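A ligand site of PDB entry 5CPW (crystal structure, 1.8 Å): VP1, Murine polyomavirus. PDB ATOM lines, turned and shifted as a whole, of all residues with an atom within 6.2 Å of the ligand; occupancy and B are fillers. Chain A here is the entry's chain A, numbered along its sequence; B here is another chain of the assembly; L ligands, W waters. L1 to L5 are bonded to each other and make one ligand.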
ATOM      1  N   GLN A  27       5.105  -5.203 -14.143  1.00  0.00           N
ATOM      2  CA  GLN A  27       4.075  -5.419 -15.159  1.00  0.00           C
ATOM      3  C   GLN A  27       3.199  -6.598 -14.733  1.00  0.00           C
ATOM      4  O   GLN A  27       3.724  -7.685 -14.475  1.00  0.00           O
ATOM      5  CB  GLN A  27       4.682  -5.665 -16.552  1.00  0.00           C
ATOM      6  CG  GLN A  27       3.622  -5.945 -17.626  1.00  0.00           C
ATOM      7  CD  GLN A  27       2.733  -4.740 -17.903  1.00  0.00           C
ATOM      8  OE1 GLN A  27       3.094  -3.605 -17.597  1.00  0.00           O
ATOM      9  NE2 GLN A  27       1.569  -4.985 -18.511  1.00  0.00           N
ATOM     10  N   SER A  33      -1.425  -9.408 -24.452  1.00  0.00           N
ATOM     11  CA  SER A  33      -0.942  -8.930 -25.748  1.00  0.00           C
ATOM     12  C   SER A  33       0.533  -8.553 -25.726  1.00  0.00           C
ATOM     13  O   SER A  33       0.983  -7.811 -24.860  1.00  0.00           O
ATOM     14  CB  SER A  33      -1.754  -7.728 -26.222  1.00  0.00           C
ATOM     15  OG  SER A  33      -1.093  -7.070 -27.285  1.00  0.00           O
ATOM     16  N   THR A  35       2.028  -6.637 -27.667  1.00  0.00           N
ATOM     17  CA  THR A  35       2.216  -5.237 -28.067  1.00  0.00           C
ATOM     18  C   THR A  35       1.617  -4.252 -27.055  1.00  0.00           C
ATOM     19  O   THR A  35       2.039  -3.089 -26.995  1.00  0.00           O
ATOM     20  CB  THR A  35       1.640  -4.933 -29.473  1.00  0.00           C
ATOM     21  OG1 THR A  35       0.226  -5.154 -29.484  1.00  0.00           O
ATOM     22  CG2 THR A  35       2.310  -5.796 -30.538  1.00  0.00           C
ATOM     23  N   GLU A  36       0.654  -4.705 -26.262  1.00  0.00           N
ATOM     24  CA  GLU A  36      -0.092  -3.818 -25.368  1.00  0.00           C
ATOM     25  C   GLU A  36       0.432  -3.810 -23.929  1.00  0.00           C
ATOM     26  O   GLU A  36      -0.254  -3.336 -23.021  1.00  0.00           O
ATOM     27  CB  GLU A  36      -1.600  -4.157 -25.398  1.00  0.00           C
ATOM     28  CG  GLU A  36      -2.283  -3.971 -26.745  1.00  0.00           C
ATOM     29  CD  GLU A  36      -2.579  -2.511 -27.076  1.00  0.00           C
ATOM     30  OE1 GLU A  36      -3.228  -2.259 -28.124  1.00  0.00           O
ATOM     31  OE2 GLU A  36      -2.174  -1.623 -26.300  1.00  0.00           O
ATOM     32  N   GLY A  37       1.655  -4.299 -23.723  1.00  0.00           N
ATOM     33  CA  GLY A  37       2.241  -4.313 -22.389  1.00  0.00           C
ATOM     34  C   GLY A  37       2.688  -5.681 -21.919  1.00  0.00           C
ATOM     35  O   GLY A  37       3.570  -5.783 -21.090  1.00  0.00           O
ATOM     36  N   GLN A  39       4.453  -7.856 -23.341  1.00  0.00           N
ATOM     37  CA  GLN A  39       5.885  -8.019 -23.613  1.00  0.00           C
ATOM     38  C   GLN A  39       6.795  -7.703 -22.393  1.00  0.00           C
ATOM     39  O   GLN A  39       7.944  -8.135 -22.357  1.00  0.00           O
ATOM     40  CB  GLN A  39       6.310  -7.217 -24.862  1.00  0.00           C
ATOM     41  CG  GLN A  39       6.299  -5.698 -24.733  1.00  0.00           C
ATOM     42  CD  GLN A  39       4.989  -5.061 -25.164  1.00  0.00           C
ATOM     43  OE1 GLN A  39       3.905  -5.521 -24.806  1.00  0.00           O
ATOM     44  NE2 GLN A  39       5.073  -3.984 -25.947  1.00  0.00           N
ATOM     45  N   TYR A  40       6.278  -6.964 -21.413  1.00  0.00           N
ATOM     46  CA  TYR A  40       7.047  -6.662 -20.196  1.00  0.00           C
ATOM     47  C   TYR A  40       6.784  -7.625 -19.039  1.00  0.00           C
ATOM     48  O   TYR A  40       7.358  -7.480 -17.956  1.00  0.00           O
ATOM     49  CB  TYR A  40       6.827  -5.199 -19.747  1.00  0.00           C
ATOM     50  CG  TYR A  40       7.122  -4.195 -20.839  1.00  0.00           C
ATOM     51  CD1 TYR A  40       8.440  -3.846 -21.166  1.00  0.00           C
ATOM     52  CD2 TYR A  40       6.093  -3.592 -21.562  1.00  0.00           C
ATOM     53  CE1 TYR A  40       8.712  -2.929 -22.168  1.00  0.00           C
ATOM     54  CE2 TYR A  40       6.353  -2.674 -22.571  1.00  0.00           C
ATOM     55  CZ  TYR A  40       7.672  -2.349 -22.878  1.00  0.00           C
ATOM     56  OH  TYR A  40       7.915  -1.440 -23.888  1.00  0.00           O
ATOM     57  N   SER A  44       9.956  -5.334 -14.869  1.00  0.00           N
ATOM     58  CA  SER A  44       9.277  -4.088 -14.526  1.00  0.00           C
ATOM     59  C   SER A  44       9.075  -3.274 -15.780  1.00  0.00           C
ATOM     60  O   SER A  44       9.651  -3.565 -16.828  1.00  0.00           O
ATOM     61  CB  SER A  44      10.101  -3.283 -13.510  1.00  0.00           C
ATOM     62  OG  SER A  44      11.218  -2.664 -14.126  1.00  0.00           O
ATOM     63  N   ARG A  45       8.270  -2.219 -15.676  1.00  0.00           N
ATOM     64  CA  ARG A  45       8.290  -1.160 -16.673  1.00  0.00           C
ATOM     65  C   ARG A  45       9.513  -0.269 -16.412  1.00  0.00           C
ATOM     66  O   ARG A  45      10.185  -0.419 -15.369  1.00  0.00           O
ATOM     67  CB  ARG A  45       6.969  -0.388 -16.635  1.00  0.00           C
ATOM     68  CG  ARG A  45       5.741  -1.248 -16.938  1.00  0.00           C
ATOM     69  CD  ARG A  45       5.801  -1.909 -18.316  1.00  0.00           C
ATOM     70  NE  ARG A  45       5.533  -0.987 -19.413  1.00  0.00           N
ATOM     71  CZ  ARG A  45       4.376  -0.895 -20.078  1.00  0.00           C
ATOM     72  NH1 ARG A  45       3.344  -1.667 -19.782  1.00  0.00           N
ATOM     73  NH2 ARG A  45       4.254  -0.014 -21.054  1.00  0.00           N
ATOM     74  N   GLY A  46       9.823   0.620 -17.357  1.00  0.00           N
ATOM     75  CA  GLY A  46      11.032   1.464 -17.274  1.00  0.00           C
ATOM     76  C   GLY A  46      11.084   2.278 -15.983  1.00  0.00           C
ATOM     77  O   GLY A  46      10.150   3.023 -15.683  1.00  0.00           O
ATOM     78  N   ILE A  47      12.168   2.128 -15.236  1.00  0.00           N
ATOM     79  CA  ILE A  47      12.312   2.799 -13.932  1.00  0.00           C
ATOM     80  C   ILE A  47      12.295   4.325 -14.122  1.00  0.00           C
ATOM     81  O   ILE A  47      13.026   4.867 -14.952  1.00  0.00           O
ATOM     82  CB  ILE A  47      13.581   2.299 -13.188  1.00  0.00           C
ATOM     83  CG1 ILE A  47      13.390   0.840 -12.740  1.00  0.00           C
ATOM     84  CG2 ILE A  47      13.922   3.195 -11.989  1.00  0.00           C
ATOM     85  CD1 ILE A  47      14.648   0.132 -12.276  1.00  0.00           C
ATOM     86  N   ASN A  48      11.416   5.008 -13.376  1.00  0.00           N
ATOM     87  CA  ASN A  48      11.290   6.456 -13.442  1.00  0.00           C
ATOM     88  C   ASN A  48      11.970   7.098 -12.234  1.00  0.00           C
ATOM     89  O   ASN A  48      11.820   6.630 -11.115  1.00  0.00           O
ATOM     90  CB  ASN A  48       9.814   6.923 -13.575  1.00  0.00           C
ATOM     91  CG  ASN A  48       8.989   6.707 -12.309  1.00  0.00           C
ATOM     92  OD1 ASN A  48       8.721   5.570 -11.891  1.00  0.00           O
ATOM     93  ND2 ASN A  48       8.557   7.806 -11.687  1.00  0.00           N
ATOM     94  N   GLU A  59       6.464   4.906 -10.018  1.00  0.00           N
ATOM     95  CA  GLU A  59       5.219   4.289 -10.494  1.00  0.00           C
ATOM     96  C   GLU A  59       5.146   2.863  -9.986  1.00  0.00           C
ATOM     97  O   GLU A  59       6.187   2.191  -9.844  1.00  0.00           O
ATOM     98  CB  GLU A  59       5.112   4.298 -12.017  1.00  0.00           C
ATOM     99  CG  GLU A  59       5.143   5.685 -12.653  1.00  0.00           C
ATOM    100  CD  GLU A  59       3.883   6.523 -12.457  1.00  0.00           C
ATOM    101  OE1 GLU A  59       2.835   6.033 -11.985  1.00  0.00           O
ATOM    102  OE2 GLU A  59       3.942   7.721 -12.821  1.00  0.00           O
ATOM    103  N   ASN A  60       3.932   2.395  -9.701  1.00  0.00           N
ATOM    104  CA  ASN A  60       3.788   1.050  -9.129  1.00  0.00           C
ATOM    105  C   ASN A  60       4.382  -0.036 -10.016  1.00  0.00           C
ATOM    106  O   ASN A  60       4.965  -0.994  -9.528  1.00  0.00           O
ATOM    107  CB  ASN A  60       2.329   0.728  -8.840  1.00  0.00           C
ATOM    108  CG  ASN A  60       1.781   1.472  -7.640  1.00  0.00           C
ATOM    109  OD1 ASN A  60       2.550   1.956  -6.802  1.00  0.00           O
ATOM    110  ND2 ASN A  60       0.469   1.551  -7.545  1.00  0.00           N
ATOM    111  N   ASN A  61       4.243   0.140 -11.331  1.00  0.00           N
ATOM    112  CA  ASN A  61       4.717  -0.892 -12.283  1.00  0.00           C
ATOM    113  C   ASN A  61       6.244  -0.880 -12.486  1.00  0.00           C
ATOM    114  O   ASN A  61       6.776  -1.613 -13.338  1.00  0.00           O
ATOM    115  CB  ASN A  61       3.930  -0.829 -13.606  1.00  0.00           C
ATOM    116  CG  ASN A  61       4.116   0.492 -14.333  1.00  0.00           C
ATOM    117  OD1 ASN A  61       4.939   1.311 -13.947  1.00  0.00           O
ATOM    118  ND2 ASN A  61       3.322   0.694 -15.385  1.00  0.00           N
ATOM    119  N   THR A  62       6.944  -0.046 -11.712  1.00  0.00           N
ATOM    120  CA  THR A  62       8.407  -0.016 -11.668  1.00  0.00           C
ATOM    121  C   THR A  62       8.965  -0.630 -10.361  1.00  0.00           C
ATOM    122  O   THR A  62      10.177  -0.711 -10.182  1.00  0.00           O
ATOM    123  CB  THR A  62       8.992   1.419 -11.826  1.00  0.00           C
ATOM    124  OG1 THR A  62       8.750   2.190 -10.634  1.00  0.00           O
ATOM    125  CG2 THR A  62       8.422   2.131 -13.040  1.00  0.00           C
ATOM    126  N   ARG A 257      17.835  -5.204 -17.242  1.00  0.00           N
ATOM    127  CA  ARG A 257      18.298  -4.972 -18.607  1.00  0.00           C
ATOM    128  C   ARG A 257      18.227  -3.468 -18.847  1.00  0.00           C
ATOM    129  O   ARG A 257      17.467  -2.749 -18.169  1.00  0.00           O
ATOM    130  CB  ARG A 257      17.498  -5.756 -19.657  1.00  0.00           C
ATOM    131  CG  ARG A 257      16.084  -5.252 -19.888  1.00  0.00           C
ATOM    132  CD  ARG A 257      15.402  -6.017 -21.020  1.00  0.00           C
ATOM    133  NE  ARG A 257      14.026  -5.583 -21.188  1.00  0.00           N
ATOM    134  CZ  ARG A 257      13.660  -4.508 -21.888  1.00  0.00           C
ATOM    135  NH1 ARG A 257      14.571  -3.770 -22.485  1.00  0.00           N
ATOM    136  NH2 ARG A 257      12.377  -4.184 -21.985  1.00  0.00           N
ATOM    137  N   THR A 259      17.932  -0.474 -21.921  1.00  0.00           N
ATOM    138  CA  THR A 259      17.546  -0.242 -23.310  1.00  0.00           C
ATOM    139  C   THR A 259      18.512   0.692 -24.043  1.00  0.00           C
ATOM    140  O   THR A 259      19.412   1.283 -23.441  1.00  0.00           O
ATOM    141  CB  THR A 259      16.109   0.337 -23.420  1.00  0.00           C
ATOM    142  OG1 THR A 259      16.139   1.732 -23.108  1.00  0.00           O
ATOM    143  CG2 THR A 259      15.155  -0.388 -22.463  1.00  0.00           C
ATOM    144  N   ASN A 261      17.540   3.401 -25.268  1.00  0.00           N
ATOM    145  CA  ASN A 261      16.924   4.734 -25.233  1.00  0.00           C
ATOM    146  C   ASN A 261      17.143   5.349 -23.858  1.00  0.00           C
ATOM    147  O   ASN A 261      16.448   4.982 -22.917  1.00  0.00           O
ATOM    148  CB  ASN A 261      15.422   4.685 -25.519  1.00  0.00           C
ATOM    149  CG  ASN A 261      15.077   3.794 -26.696  1.00  0.00           C
ATOM    150  OD1 ASN A 261      15.532   4.027 -27.815  1.00  0.00           O
ATOM    151  ND2 ASN A 261      14.264   2.757 -26.443  1.00  0.00           N
ATOM    152  N   VAL A 264      17.255   3.359 -20.182  1.00  0.00           N
ATOM    153  CA  VAL A 264      16.123   2.957 -19.349  1.00  0.00           C
ATOM    154  C   VAL A 264      16.363   1.545 -18.793  1.00  0.00           C
ATOM    155  O   VAL A 264      16.712   0.620 -19.532  1.00  0.00           O
ATOM    156  CB  VAL A 264      14.775   3.048 -20.110  1.00  0.00           C
ATOM    157  CG1 VAL A 264      13.660   2.395 -19.311  1.00  0.00           C
ATOM    158  CG2 VAL A 264      14.433   4.505 -20.392  1.00  0.00           C
ATOM    159  N   HIS A 266      15.028  -1.921 -16.794  1.00  0.00           N
ATOM    160  CA  HIS A 266      13.879  -2.775 -16.431  1.00  0.00           C
ATOM    161  C   HIS A 266      14.371  -3.902 -15.524  1.00  0.00           C
ATOM    162  O   HIS A 266      15.286  -4.649 -15.888  1.00  0.00           O
ATOM    163  CB  HIS A 266      13.220  -3.412 -17.673  1.00  0.00           C
ATOM    164  CG  HIS A 266      12.603  -2.429 -18.621  1.00  0.00           C
ATOM    165  ND1 HIS A 266      11.240  -2.247 -18.723  1.00  0.00           N
ATOM    166  CD2 HIS A 266      13.163  -1.618 -19.556  1.00  0.00           C
ATOM    167  CE1 HIS A 266      10.989  -1.341 -19.658  1.00  0.00           C
ATOM    168  NE2 HIS A 266      12.139  -0.948 -20.179  1.00  0.00           N
ATOM    169  N   ASP B  53      13.117  -3.457 -31.605  1.00  0.00           N
ATOM    170  CA  ASP B  53      12.404  -4.047 -30.471  1.00  0.00           C
ATOM    171  C   ASP B  53      11.431  -5.170 -30.887  1.00  0.00           C
ATOM    172  O   ASP B  53      11.041  -5.989 -30.069  1.00  0.00           O
ATOM    173  CB  ASP B  53      11.622  -2.945 -29.736  1.00  0.00           C
ATOM    174  CG  ASP B  53      10.742  -3.483 -28.618  1.00  0.00           C
ATOM    175  OD1 ASP B  53      11.273  -4.052 -27.643  1.00  0.00           O
ATOM    176  OD2 ASP B  53       9.497  -3.307 -28.710  1.00  0.00           O
ATOM    177  N   ARG B 150       8.640 -12.679 -28.050  1.00  0.00           N
ATOM    178  CA  ARG B 150       8.531 -12.144 -29.414  1.00  0.00           C
ATOM    179  C   ARG B 150       9.695 -12.592 -30.298  1.00  0.00           C
ATOM    180  O   ARG B 150       9.667 -12.354 -31.511  1.00  0.00           O
ATOM    181  CB  ARG B 150       8.461 -10.617 -29.406  1.00  0.00           C
ATOM    182  CG  ARG B 150       7.270 -10.053 -28.648  1.00  0.00           C
ATOM    183  CD  ARG B 150       7.389  -8.542 -28.474  1.00  0.00           C
ATOM    184  NE  ARG B 150       8.643  -8.197 -27.806  1.00  0.00           N
ATOM    185  CZ  ARG B 150       9.126  -6.960 -27.708  1.00  0.00           C
ATOM    186  NH1 ARG B 150       8.451  -5.940 -28.225  1.00  0.00           N
ATOM    187  NH2 ARG B 150      10.293  -6.761 -27.115  1.00  0.00           N
HETATM  188  C1  LIG L   1       0.134  11.621 -22.334  1.00  0.00           C
HETATM  189  C2  LIG L   1       0.241  10.125 -22.659  1.00  0.00           C
HETATM  190  C3  LIG L   1      -0.368   9.269 -21.542  1.00  0.00           C
HETATM  191  C4  LIG L   1       0.257   9.675 -20.206  1.00  0.00           C
HETATM  192  C5  LIG L   1      -0.025  11.162 -20.005  1.00  0.00           C
HETATM  193  C6  LIG L   1       0.452  11.687 -18.648  1.00  0.00           C
HETATM  194  O1  LIG L   1       0.893  12.382 -23.252  1.00  0.00           O
HETATM  195  O2  LIG L   1      -0.420   9.836 -23.873  1.00  0.00           O
HETATM  196  O3  LIG L   1      -0.195   7.899 -21.828  1.00  0.00           O
HETATM  197  O4  LIG L   1       1.657   9.475 -20.238  1.00  0.00           O
HETATM  198  O5  LIG L   1       0.615  11.897 -21.032  1.00  0.00           O
HETATM  199  O6  LIG L   1      -0.512  11.387 -17.662  1.00  0.00           O
HETATM  200  C1  LG2 L   2       2.057   8.450 -19.324  1.00  0.00           C
HETATM  201  C2  LG2 L   2       3.438   7.918 -19.731  1.00  0.00           C
HETATM  202  C3  LG2 L   2       4.056   7.007 -18.662  1.00  0.00           C
HETATM  203  C4  LG2 L   2       3.904   7.607 -17.266  1.00  0.00           C
HETATM  204  C5  LG2 L   2       2.436   7.938 -17.042  1.00  0.00           C
HETATM  205  C6  LG2 L   2       2.135   8.454 -15.637  1.00  0.00           C
HETATM  206  C7  LG2 L   2       3.698   7.776 -22.177  1.00  0.00           C
HETATM  207  C8  LG2 L   2       3.571   6.887 -23.385  1.00  0.00           C
HETATM  208  N1  LG2 L   2       3.378   7.220 -21.013  1.00  0.00           N
HETATM  209  O1  LG2 L   2       5.440   6.832 -18.991  1.00  0.00           O
HETATM  210  O2  LG2 L   2       4.701   8.795 -17.177  1.00  0.00           O
HETATM  211  O3  LG2 L   2       2.068   8.948 -17.984  1.00  0.00           O
HETATM  212  O4  LG2 L   2       0.715   8.334 -15.427  1.00  0.00           O
HETATM  213  O5  LG2 L   2       4.069   8.937 -22.295  1.00  0.00           O
HETATM  214  C1  LG3 L   3       5.805   5.446 -18.884  1.00  0.00           C
HETATM  215  C2  LG3 L   3       7.052   5.215 -19.727  1.00  0.00           C
HETATM  216  C3  LG3 L   3       7.512   3.760 -19.570  1.00  0.00           C
HETATM  217  C4  LG3 L   3       7.707   3.435 -18.087  1.00  0.00           C
HETATM  218  C5  LG3 L   3       6.424   3.752 -17.321  1.00  0.00           C
HETATM  219  C6  LG3 L   3       6.570   3.513 -15.823  1.00  0.00           C
HETATM  220  O1  LG3 L   3       6.767   5.471 -21.086  1.00  0.00           O
HETATM  221  O2  LG3 L   3       8.711   3.549 -20.314  1.00  0.00           O
HETATM  222  O3  LG3 L   3       8.791   4.213 -17.590  1.00  0.00           O
HETATM  223  O4  LG3 L   3       6.028   5.097 -17.521  1.00  0.00           O
HETATM  224  O5  LG3 L   3       5.302   3.669 -15.194  1.00  0.00           O
HETATM  225  C1  LG4 L   4       7.826   1.226 -20.639  1.00  0.00           C
HETATM  226  C2  LG4 L   4       8.706   2.360 -21.137  1.00  0.00           C
HETATM  227  C3  LG4 L   4      10.175   1.939 -21.215  1.00  0.00           C
HETATM  228  C4  LG4 L   4      10.370   0.923 -22.349  1.00  0.00           C
HETATM  229  C5  LG4 L   4       9.830   1.465 -23.686  1.00  0.00           C
HETATM  230  C6  LG4 L   4       8.379   1.912 -23.508  1.00  0.00           C
HETATM  231  C7  LG4 L   4       7.795   2.568 -24.766  1.00  0.00           C
HETATM  232  C8  LG4 L   4       6.266   2.630 -24.724  1.00  0.00           C
HETATM  233  C9  LG4 L   4       5.693   3.851 -24.011  1.00  0.00           C
HETATM  234  C10 LG4 L   4      10.545   0.686 -25.894  1.00  0.00           C
HETATM  235  C11 LG4 L   4      10.544  -0.459 -26.864  1.00  0.00           C
HETATM  236  N1  LG4 L   4       9.930   0.451 -24.729  1.00  0.00           N
HETATM  237  O1  LG4 L   4       8.241   0.519 -19.704  1.00  0.00           O
HETATM  238  O2  LG4 L   4       6.710   1.015 -21.182  1.00  0.00           O
HETATM  239  O3  LG4 L   4      11.770   0.626 -22.468  1.00  0.00           O
HETATM  240  O4  LG4 L   4       8.270   2.839 -22.423  1.00  0.00           O
HETATM  241  O5  LG4 L   4       8.391   3.863 -24.954  1.00  0.00           O
HETATM  242  O6  LG4 L   4       5.800   2.614 -26.085  1.00  0.00           O
HETATM  243  O7  LG4 L   4       4.338   3.587 -23.647  1.00  0.00           O
HETATM  244  O8  LG4 L   4      11.102   1.750 -26.159  1.00  0.00           O
HETATM  245  C1  LG5 L   5       6.004   0.180 -26.143  1.00  0.00           C
HETATM  246  C2  LG5 L   5       5.145   1.396 -26.497  1.00  0.00           C
HETATM  247  C3  LG5 L   5       4.953   1.536 -28.019  1.00  0.00           C
HETATM  248  C4  LG5 L   5       3.953   0.530 -28.590  1.00  0.00           C
HETATM  249  C5  LG5 L   5       2.652   0.512 -27.788  1.00  0.00           C
HETATM  250  C6  LG5 L   5       2.984   0.289 -26.308  1.00  0.00           C
HETATM  251  C7  LG5 L   5       1.760   0.272 -25.399  1.00  0.00           C
HETATM  252  C8  LG5 L   5       2.158   0.216 -23.913  1.00  0.00           C
HETATM  253  C9  LG5 L   5       1.001  -0.225 -23.033  1.00  0.00           C
HETATM  254  C10 LG5 L   5       0.707  -0.226 -29.052  1.00  0.00           C
HETATM  255  C11 LG5 L   5      -0.136  -1.396 -29.474  1.00  0.00           C
HETATM  256  N1  LG5 L   5       1.743  -0.517 -28.280  1.00  0.00           N
HETATM  257  O1  LG5 L   5       6.946  -0.126 -26.894  1.00  0.00           O
HETATM  258  O2  LG5 L   5       5.757  -0.480 -25.093  1.00  0.00           O
HETATM  259  O3  LG5 L   5       3.673   0.878 -29.954  1.00  0.00           O
HETATM  260  O4  LG5 L   5       3.873   1.314 -25.852  1.00  0.00           O
HETATM  261  O5  LG5 L   5       0.974   1.454 -25.632  1.00  0.00           O
HETATM  262  O6  LG5 L   5       3.242  -0.717 -23.755  1.00  0.00           O
HETATM  263  O7  LG5 L   5       1.338   0.059 -21.669  1.00  0.00           O
HETATM  264  O8  LG5 L   5       0.462   0.921 -29.402  1.00  0.00           O
HETATM  265  O   HOH W   1       7.567  -2.831 -26.639  1.00  0.00           O
HETATM  266  O   HOH W   2      -1.375   0.827 -26.618  1.00  0.00           O
HETATM  267  O   HOH W   3       5.855   8.726 -14.609  1.00  0.00           O
HETATM  268  O   HOH W   4       7.080   8.361 -21.149  1.00  0.00           O
HETATM  269  O   HOH W   5       8.787   5.596 -22.960  1.00  0.00           O
HETATM  270  O   HOH W   6       7.082   9.258 -18.663  1.00  0.00           O
HETATM  271  O   HOH W   7      11.056   4.806 -19.188  1.00  0.00           O
HETATM  272  O   HOH W   8       3.412  11.437 -21.020  1.00  0.00           O
HETATM  273  O   HOH W   9       2.920   4.495 -16.343  1.00  0.00           O
HETATM  274  O   HOH W  10      11.449   2.626 -28.815  1.00  0.00           O
HETATM  275  O   HOH W  11       2.203   3.873 -25.184  1.00  0.00           O
HETATM  276  O   HOH W  12       8.194   1.018 -29.040  1.00  0.00           O
HETATM  277  O   HOH W  13      13.539   2.451 -23.436  1.00  0.00           O
HETATM  278  O   HOH W  14      12.082  -1.841 -23.932  1.00  0.00           O
HETATM  279  O   HOH W  15       0.881   5.745 -14.082  1.00  0.00           O
HETATM  280  O   HOH W  16       7.611   7.067 -16.248  1.00  0.00           O
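Water W2 lies within hydrogen-bond range of OE2 of Glu 36 (2.6 Å) and O5 of LG5 L5 (2.6 Å).
Water W13 lies within hydrogen-bond range of OG1 of Thr 259, O3 of LG4 L4 and ND2 of Asn 261.
Water W1 lies within hydrogen-bond range of an oxygen (O1) of LG5 L5, the side-chain amide nitrogen of Gln 39, the side-chain carboxylate of Asp 53 of chain B and the side-chain hydroxyl of Tyr 40.
Water W3 lies within hydrogen-bond range of OE2 of Glu 59 (2.8 Å) and O2 of LG2 L2 (2.8 Å).
Water W14 lies within hydrogen-bond range of O3 of LG4 L4 (2.9 Å) and NH2 of Arg 257 (3.1 Å).
Water W15 bridges OE1 of Glu 59 (2.9 Å) and O4 of LG2 L2 (2.9 Å).
O1 of LG4 L4 sits at hydrogen-bond distance from N of Gly 46, at 2.8 Å.
The backbone carbonyl oxygen (O) of Gly 46 lies within hydrogen-bond range of an oxygen (O3) of LG3 L3 (2.6 Å).
O2 of LG5 L5 lies within hydrogen-bond range of OH of Tyr 40, 2.7 Å away.
The guanidinium group (NH2) of Arg 45 is in salt-bridge range of an oxygen (O2) of LG4 L4.
OD1 of Asn 61 lies within hydrogen-bond range of O5 of LG3 L3 (2.7 Å).
An oxygen (O3) of LG4 L4 lies within hydrogen-bond range of a ring nitrogen (NE2) of His 266 (2.8 Å).
The backbone carbonyl oxygen (O) of Thr 35 is in hydrogen-bond range of a nitrogen (N1) of LG5 L5 (2.9 Å).
The side-chain amide nitrogen (ND2) of Asn 261 sits at hydrogen-bond distance from an oxygen (O8) of LG4 L4 (3.3 Å).
Glu 36 touches the ligand.
N of Gly 37 touches O6 of LG5 L5, 3.9 Å away.
NE2 of Gln 39 touches O2 of LG5 L5, at 3.7 Å.
CB of Glu 59 touches O5 of LG3 L3, at 3.2 Å.
Thr 62 touches the ligand.
CG2 of Thr 259 touches O3 of LG4 L4 (3.5 Å).
CG1 of Val 264 touches C3 of LG4 L4, 3.997 Å away.
Asp 53 of chain B touches the ligand.
Of the 23 residues printed, 15 come within 4 Å of the ligand.
The nearest printed residue that does not touch the ligand is Ile 47 (4.6 Å).
The backbone NH (N) of Arg 45 lies within hydrogen-bond range of the backbone carbonyl oxygen (O) of Asn 61, at 2.8 Å.
O of Ser 44 lies within hydrogen-bond range of ND1 of His 266.
The backbone carbonyl oxygen (O) of Glu 59 lies within hydrogen-bond range of the side-chain hydroxyl (OG1) of Thr 62.
The side-chain amide oxygen (OD1) of Asn 48 sits at hydrogen-bond distance from the backbone NH (N) of Glu 59, at 3.0 Å.
OG1 of Thr 259 is in hydrogen-bond range of N of Asn 261 (3.1 Å).
The guanidinium group (NH1) of Arg 150 of chain B lies within salt-bridge range of the side-chain carboxylate (OD2) of Asp 53 of chain B (2.9 Å).
N of Thr 259 is in hydrogen-bond range of O of Val 264 (2.9 Å).
The backbone NH (N) of Gly 37 is in hydrogen-bond range of the side-chain amide oxygen (OE1) of Gln 39, 2.8 Å away.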
